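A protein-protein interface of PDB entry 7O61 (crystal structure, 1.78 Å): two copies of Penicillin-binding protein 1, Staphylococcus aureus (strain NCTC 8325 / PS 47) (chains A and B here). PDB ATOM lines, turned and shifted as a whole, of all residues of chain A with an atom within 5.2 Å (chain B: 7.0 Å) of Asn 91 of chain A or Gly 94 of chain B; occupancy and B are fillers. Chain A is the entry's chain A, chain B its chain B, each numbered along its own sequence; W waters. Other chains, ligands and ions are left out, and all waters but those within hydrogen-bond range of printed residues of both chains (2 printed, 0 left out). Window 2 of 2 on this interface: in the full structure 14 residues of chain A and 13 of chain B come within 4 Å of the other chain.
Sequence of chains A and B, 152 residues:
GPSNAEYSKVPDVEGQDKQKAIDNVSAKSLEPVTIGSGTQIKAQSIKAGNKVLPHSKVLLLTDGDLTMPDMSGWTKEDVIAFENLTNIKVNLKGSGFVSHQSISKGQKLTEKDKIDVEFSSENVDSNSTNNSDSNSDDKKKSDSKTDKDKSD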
ATOM      1  N   LYS A  89     -33.959 -32.941 -22.195  1.00  0.00           N
ATOM      2  CA  LYS A  89     -32.881 -32.122 -22.724  1.00  0.00           C
ATOM      3  C   LYS A  89     -32.280 -32.781 -23.954  1.00  0.00           C
ATOM      4  O   LYS A  89     -31.966 -33.976 -23.945  1.00  0.00           O
ATOM      5  CB  LYS A  89     -31.804 -31.893 -21.662  1.00  0.00           C
ATOM      6  N   VAL A  90     -32.128 -32.003 -25.018  1.00  0.00           N
ATOM      7  CA  VAL A  90     -31.479 -32.464 -26.235  1.00  0.00           C
ATOM      8  C   VAL A  90     -30.219 -31.640 -26.445  1.00  0.00           C
ATOM      9  O   VAL A  90     -30.264 -30.404 -26.406  1.00  0.00           O
ATOM     10  CB  VAL A  90     -32.399 -32.350 -27.461  1.00  0.00           C
ATOM     11  CG1 VAL A  90     -31.687 -32.908 -28.685  1.00  0.00           C
ATOM     12  CG2 VAL A  90     -33.714 -33.073 -27.214  1.00  0.00           C
ATOM     13  N   ASN A  91     -29.097 -32.322 -26.648  1.00  0.00           N
ATOM     14  CA  ASN A  91     -27.853 -31.658 -27.012  1.00  0.00           C
ATOM     15  C   ASN A  91     -27.743 -31.646 -28.531  1.00  0.00           C
ATOM     16  O   ASN A  91     -27.765 -32.702 -29.171  1.00  0.00           O
ATOM     17  CB  ASN A  91     -26.652 -32.349 -26.370  1.00  0.00           C
ATOM     18  CG  ASN A  91     -26.549 -32.067 -24.884  1.00  0.00           C
ATOM     19  OD1 ASN A  91     -26.977 -31.011 -24.411  1.00  0.00           O
ATOM     20  ND2 ASN A  91     -25.981 -33.008 -24.139  1.00  0.00           N
ATOM     21  N   LEU A  92     -27.652 -30.451 -29.104  1.00  0.00           N
ATOM     22  CA  LEU A  92     -27.644 -30.263 -30.548  1.00  0.00           C
ATOM     23  C   LEU A  92     -26.212 -30.032 -31.008  1.00  0.00           C
ATOM     24  O   LEU A  92     -25.559 -29.083 -30.563  1.00  0.00           O
ATOM     25  CB  LEU A  92     -28.538 -29.085 -30.944  1.00  0.00           C
ATOM     26  CG  LEU A  92     -30.044 -29.271 -30.750  1.00  0.00           C
ATOM     27  CD1 LEU A  92     -30.469 -28.893 -29.339  1.00  0.00           C
ATOM     28  CD2 LEU A  92     -30.809 -28.445 -31.772  1.00  0.00           C
ATOM     29  N   LYS A  93     -25.726 -30.898 -31.894  1.00  0.00           N
ATOM     30  CA  LYS A  93     -24.351 -30.836 -32.377  1.00  0.00           C
ATOM     31  C   LYS A  93     -24.362 -30.542 -33.870  1.00  0.00           C
ATOM     32  O   LYS A  93     -24.856 -31.351 -34.664  1.00  0.00           O
ATOM     33  CB  LYS A  93     -23.608 -32.143 -32.083  1.00  0.00           C
ATOM     34  N   ILE A 115     -30.765 -36.768 -24.669  1.00  0.00           N
ATOM     35  CA  ILE A 115     -30.673 -37.127 -26.078  1.00  0.00           C
ATOM     36  C   ILE A 115     -29.593 -36.277 -26.728  1.00  0.00           C
ATOM     37  O   ILE A 115     -29.572 -35.054 -26.558  1.00  0.00           O
ATOM     38  CB  ILE A 115     -32.021 -36.935 -26.794  1.00  0.00           C
ATOM     39  CG1 ILE A 115     -33.075 -37.877 -26.213  1.00  0.00           C
ATOM     40  CG2 ILE A 115     -31.874 -37.193 -28.281  1.00  0.00           C
ATOM     41  CD1 ILE A 115     -34.461 -37.602 -26.737  1.00  0.00           C
ATOM     42  N   ASP A 116     -28.692 -36.927 -27.460  1.00  0.00           N
ATOM     43  CA  ASP A 116     -27.749 -36.234 -28.324  1.00  0.00           C
ATOM     44  C   ASP A 116     -28.224 -36.354 -29.765  1.00  0.00           C
ATOM     45  O   ASP A 116     -28.546 -37.451 -30.230  1.00  0.00           O
ATOM     46  CB  ASP A 116     -26.330 -36.792 -28.185  1.00  0.00           C
ATOM     47  CG  ASP A 116     -25.758 -36.601 -26.792  1.00  0.00           C
ATOM     48  OD1 ASP A 116     -26.042 -35.558 -26.169  1.00  0.00           O
ATOM     49  OD2 ASP A 116     -25.005 -37.483 -26.326  1.00  0.00           O
ATOM     50  N   VAL A 117     -28.276 -35.226 -30.460  1.00  0.00           N
ATOM     51  CA  VAL A 117     -28.665 -35.171 -31.862  1.00  0.00           C
ATOM     52  C   VAL A 117     -27.606 -34.375 -32.608  1.00  0.00           C
ATOM     53  O   VAL A 117     -27.176 -33.318 -32.135  1.00  0.00           O
ATOM     54  CB  VAL A 117     -30.055 -34.532 -32.040  1.00  0.00           C
ATOM     55  CG1 VAL A 117     -30.386 -34.395 -33.505  1.00  0.00           C
ATOM     56  CG2 VAL A 117     -31.114 -35.372 -31.340  1.00  0.00           C
ATOM     57  N   GLU A 118     -27.179 -34.880 -33.762  1.00  0.00           N
ATOM     58  CA  GLU A 118     -26.229 -34.164 -34.595  1.00  0.00           C
ATOM     59  C   GLU A 118     -26.816 -33.918 -35.980  1.00  0.00           C
ATOM     60  O   GLU A 118     -27.678 -34.664 -36.457  1.00  0.00           O
ATOM     61  CB  GLU A 118     -24.889 -34.906 -34.680  1.00  0.00           C
ATOM     62  CG  GLU A 118     -24.942 -36.303 -35.240  1.00  0.00           C
ATOM     63  CD  GLU A 118     -23.578 -36.973 -35.216  1.00  0.00           C
ATOM     64  OE1 GLU A 118     -22.603 -36.315 -34.796  1.00  0.00           O
ATOM     65  OE2 GLU A 118     -23.479 -38.154 -35.609  1.00  0.00           O
ATOM     66  N   LYS B  76     -32.665 -21.643 -25.960  1.00  0.00           N
ATOM     67  CA  LYS B  76     -32.354 -22.241 -27.254  1.00  0.00           C
ATOM     68  C   LYS B  76     -33.293 -21.719 -28.331  1.00  0.00           C
ATOM     69  O   LYS B  76     -32.867 -21.427 -29.455  1.00  0.00           O
ATOM     70  CB  LYS B  76     -32.441 -23.762 -27.161  1.00  0.00           C
ATOM     71  CG  LYS B  76     -31.320 -24.391 -26.370  1.00  0.00           C
ATOM     72  CD  LYS B  76     -31.070 -25.823 -26.818  1.00  0.00           C
ATOM     73  CE  LYS B  76     -30.301 -26.595 -25.764  1.00  0.00           C
ATOM     74  NZ  LYS B  76     -31.010 -27.822 -25.317  1.00  0.00           N
ATOM     75  N   LEU B  92     -25.064 -24.513 -30.725  1.00  0.00           N
ATOM     76  CA  LEU B  92     -25.556 -24.505 -29.356  1.00  0.00           C
ATOM     77  C   LEU B  92     -24.846 -25.606 -28.579  1.00  0.00           C
ATOM     78  O   LEU B  92     -24.899 -26.770 -28.985  1.00  0.00           O
ATOM     79  CB  LEU B  92     -27.068 -24.768 -29.342  1.00  0.00           C
ATOM     80  CG  LEU B  92     -27.929 -24.117 -30.426  1.00  0.00           C
ATOM     81  CD1 LEU B  92     -29.409 -24.335 -30.164  1.00  0.00           C
ATOM     82  CD2 LEU B  92     -27.652 -22.644 -30.543  1.00  0.00           C
ATOM     83  N   LYS B  93     -24.223 -25.257 -27.455  1.00  0.00           N
ATOM     84  CA  LYS B  93     -23.480 -26.221 -26.646  1.00  0.00           C
ATOM     85  C   LYS B  93     -24.175 -26.350 -25.300  1.00  0.00           C
ATOM     86  O   LYS B  93     -24.332 -25.354 -24.588  1.00  0.00           O
ATOM     87  CB  LYS B  93     -22.018 -25.801 -26.461  1.00  0.00           C
ATOM     88  N   GLY B  94     -24.635 -27.556 -24.977  1.00  0.00           N
ATOM     89  CA  GLY B  94     -25.295 -27.789 -23.711  1.00  0.00           C
ATOM     90  C   GLY B  94     -26.742 -27.337 -23.709  1.00  0.00           C
ATOM     91  O   GLY B  94     -27.344 -27.017 -24.739  1.00  0.00           O
ATOM     92  N   SER B  95     -27.307 -27.314 -22.505  1.00  0.00           N
ATOM     93  CA  SER B  95     -28.687 -26.912 -22.291  1.00  0.00           C
ATOM     94  C   SER B  95     -28.753 -25.904 -21.154  1.00  0.00           C
ATOM     95  O   SER B  95     -27.814 -25.755 -20.368  1.00  0.00           O
ATOM     96  CB  SER B  95     -29.585 -28.120 -21.983  1.00  0.00           C
ATOM     97  OG  SER B  95     -29.579 -29.044 -23.056  1.00  0.00           O
ATOM     98  N   GLY B  96     -29.881 -25.201 -21.087  1.00  0.00           N
ATOM     99  CA  GLY B  96     -30.087 -24.193 -20.068  1.00  0.00           C
ATOM    100  C   GLY B  96     -30.278 -22.804 -20.642  1.00  0.00           C
ATOM    101  O   GLY B  96     -31.140 -22.591 -21.500  1.00  0.00           O
ATOM    102  N   VAL B 117     -22.512 -20.635 -29.056  1.00  0.00           N
ATOM    103  CA  VAL B 117     -23.083 -20.227 -27.781  1.00  0.00           C
ATOM    104  C   VAL B 117     -23.064 -21.414 -26.830  1.00  0.00           C
ATOM    105  O   VAL B 117     -23.190 -22.573 -27.237  1.00  0.00           O
ATOM    106  CB  VAL B 117     -24.509 -19.646 -27.923  1.00  0.00           C
ATOM    107  CG1 VAL B 117     -24.530 -18.548 -28.971  1.00  0.00           C
ATOM    108  CG2 VAL B 117     -25.495 -20.731 -28.287  1.00  0.00           C
ATOM    109  N   GLU B 118     -22.873 -21.113 -25.551  1.00  0.00           N
ATOM    110  CA  GLU B 118     -22.843 -22.117 -24.501  1.00  0.00           C
ATOM    111  C   GLU B 118     -23.999 -21.870 -23.548  1.00  0.00           C
ATOM    112  O   GLU B 118     -24.298 -20.722 -23.204  1.00  0.00           O
ATOM    113  CB  GLU B 118     -21.522 -22.086 -23.735  1.00  0.00           C
ATOM    114  CG  GLU B 118     -20.420 -22.906 -24.371  1.00  0.00           C
ATOM    115  CD  GLU B 118     -19.053 -22.547 -23.831  1.00  0.00           C
ATOM    116  OE1 GLU B 118     -18.076 -22.588 -24.608  1.00  0.00           O
ATOM    117  OE2 GLU B 118     -18.957 -22.225 -22.627  1.00  0.00           O
ATOM    118  N   PHE B 119     -24.650 -22.948 -23.133  1.00  0.00           N
ATOM    119  CA  PHE B 119     -25.766 -22.871 -22.208  1.00  0.00           C
ATOM    120  C   PHE B 119     -25.381 -23.473 -20.864  1.00  0.00           C
ATOM    121  O   PHE B 119     -24.540 -24.374 -20.782  1.00  0.00           O
ATOM    122  CB  PHE B 119     -26.998 -23.591 -22.757  1.00  0.00           C
ATOM    123  CG  PHE B 119     -27.582 -22.958 -23.987  1.00  0.00           C
ATOM    124  CD1 PHE B 119     -27.044 -23.206 -25.238  1.00  0.00           C
ATOM    125  CD2 PHE B 119     -28.683 -22.122 -23.890  1.00  0.00           C
ATOM    126  CE1 PHE B 119     -27.591 -22.632 -26.368  1.00  0.00           C
ATOM    127  CE2 PHE B 119     -29.236 -21.544 -25.018  1.00  0.00           C
ATOM    128  CZ  PHE B 119     -28.687 -21.797 -26.258  1.00  0.00           C
ATOM    129  N   SER B 120     -26.013 -22.964 -19.809  1.00  0.00           N
ATOM    130  CA  SER B 120     -25.791 -23.462 -18.461  1.00  0.00           C
ATOM    131  C   SER B 120     -27.074 -23.294 -17.661  1.00  0.00           C
ATOM    132  O   SER B 120     -27.979 -22.550 -18.050  1.00  0.00           O
ATOM    133  CB  SER B 120     -24.631 -22.736 -17.774  1.00  0.00           C
ATOM    134  OG  SER B 120     -25.015 -21.425 -17.398  1.00  0.00           O
HETATM  135  O   HOH W   1     -25.821 -26.817 -32.531  1.00  0.00           O
HETATM  136  O   HOH W   2     -27.250 -28.101 -27.969  1.00  0.00           O
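The backbone carbonyl oxygen of Val 90 of chain A is in hydrogen-bond range of the side-chain amino group of Lys 76 of chain B.
The backbone carbonyl oxygen (O) of Leu 92 of chain A lies close to the backbone carbonyl oxygen (O) of Leu 92 of chain B.
The backbone NH (N) of Ile 115 of chain A sits at hydrogen-bond distance from the backbone carbonyl oxygen (O) of Lys 89 of chain A (3.1 Å).
N of Asn 91 of chain A is in hydrogen-bond range of O of Ile 115 of chain A (2.8 Å).
The side-chain amide nitrogen of Asn 91 of chain A is in hydrogen-bond range of the side-chain carboxylate of Asp 116 of chain A (3.3 Å).
The backbone carbonyl oxygen (O) of Asn 91 of chain A lies within hydrogen-bond range of the backbone NH (N) of Val 117 of chain A (2.9 Å).
NZ of Lys 76 of chain B is in hydrogen-bond range of OG of Ser 95 of chain B, 2.9 Å away.
The backbone carbonyl oxygen of Ser 95 of chain B is in hydrogen-bond range of the backbone NH of Ser 120 of chain B, at 3.4 Å.
Ser 95 of chain B touches Lys 89 of chain A (OG to CB, 3.9 Å).
Val 90 of chain A touches Ser 95 of chain B.
OD1 of Asn 91 of chain A touches CA of Gly 94 of chain B, at 3.7 Å.
Asn 91 of chain A touches Ser 95 of chain B (OD1 to OG, 3.5 Å).
Printed residues of chain B within 4 Å of Asn 91 of chain A: Gly 94 and Ser 95.
Printed residues of chain A within 4 Å of Gly 94 of chain B: Asn 91.
Printed residues of chain B within 4 Å of Val 90 of chain A: Lys 76 (2.9 Å) and Ser 95 (3.7 Å).
Printed residues of chain B within 4 Å of Leu 92 of chain A: Leu 92.
Val 117 of chain B touches none of the printed residues of chain A.
The nearest printed residue of chain A that does not touch Gly 94 of chain B is Val 90 of chain A (4.8 Å).
The nearest printed residue of chain B that does not touch Leu 92 of chain A is Lys 76 of chain B (4.02 Å).
Of the 9 printed residues of chain A, 4 touch a printed residue of chain B.
Printed residues of chain A that touch a printed residue of chain B: Lys 89, Val 90, Asn 91 and Leu 92.
Of the 10 printed residues of chain B, 4 touch a printed residue of chain A.
Among the printed residues, no Asp or Glu carboxylate lies within 4 Å of a Lys or Arg side-chain nitrogen of the other chain.
Leu 92 of chain B touches its own counterpart, Leu 92 of chain A.
4 positions are printed for both chains.
Of the 6 pairs that touch across the chains among the printed residues, 1 has its exchanged pair printed and touching as well.
Water W2 lies within hydrogen-bond range of the backbone NH of Leu 92 of chain A (2.6 Å), the backbone carbonyl oxygen of Leu 92 of chain B (2.9 Å) and the backbone carbonyl oxygen of Gly 94 of chain B (3.4 Å).
Water W1 bridges the backbone carbonyl oxygen (O) of Leu 92 of chain A and the backbone NH (N) of Leu 92 of chain B.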
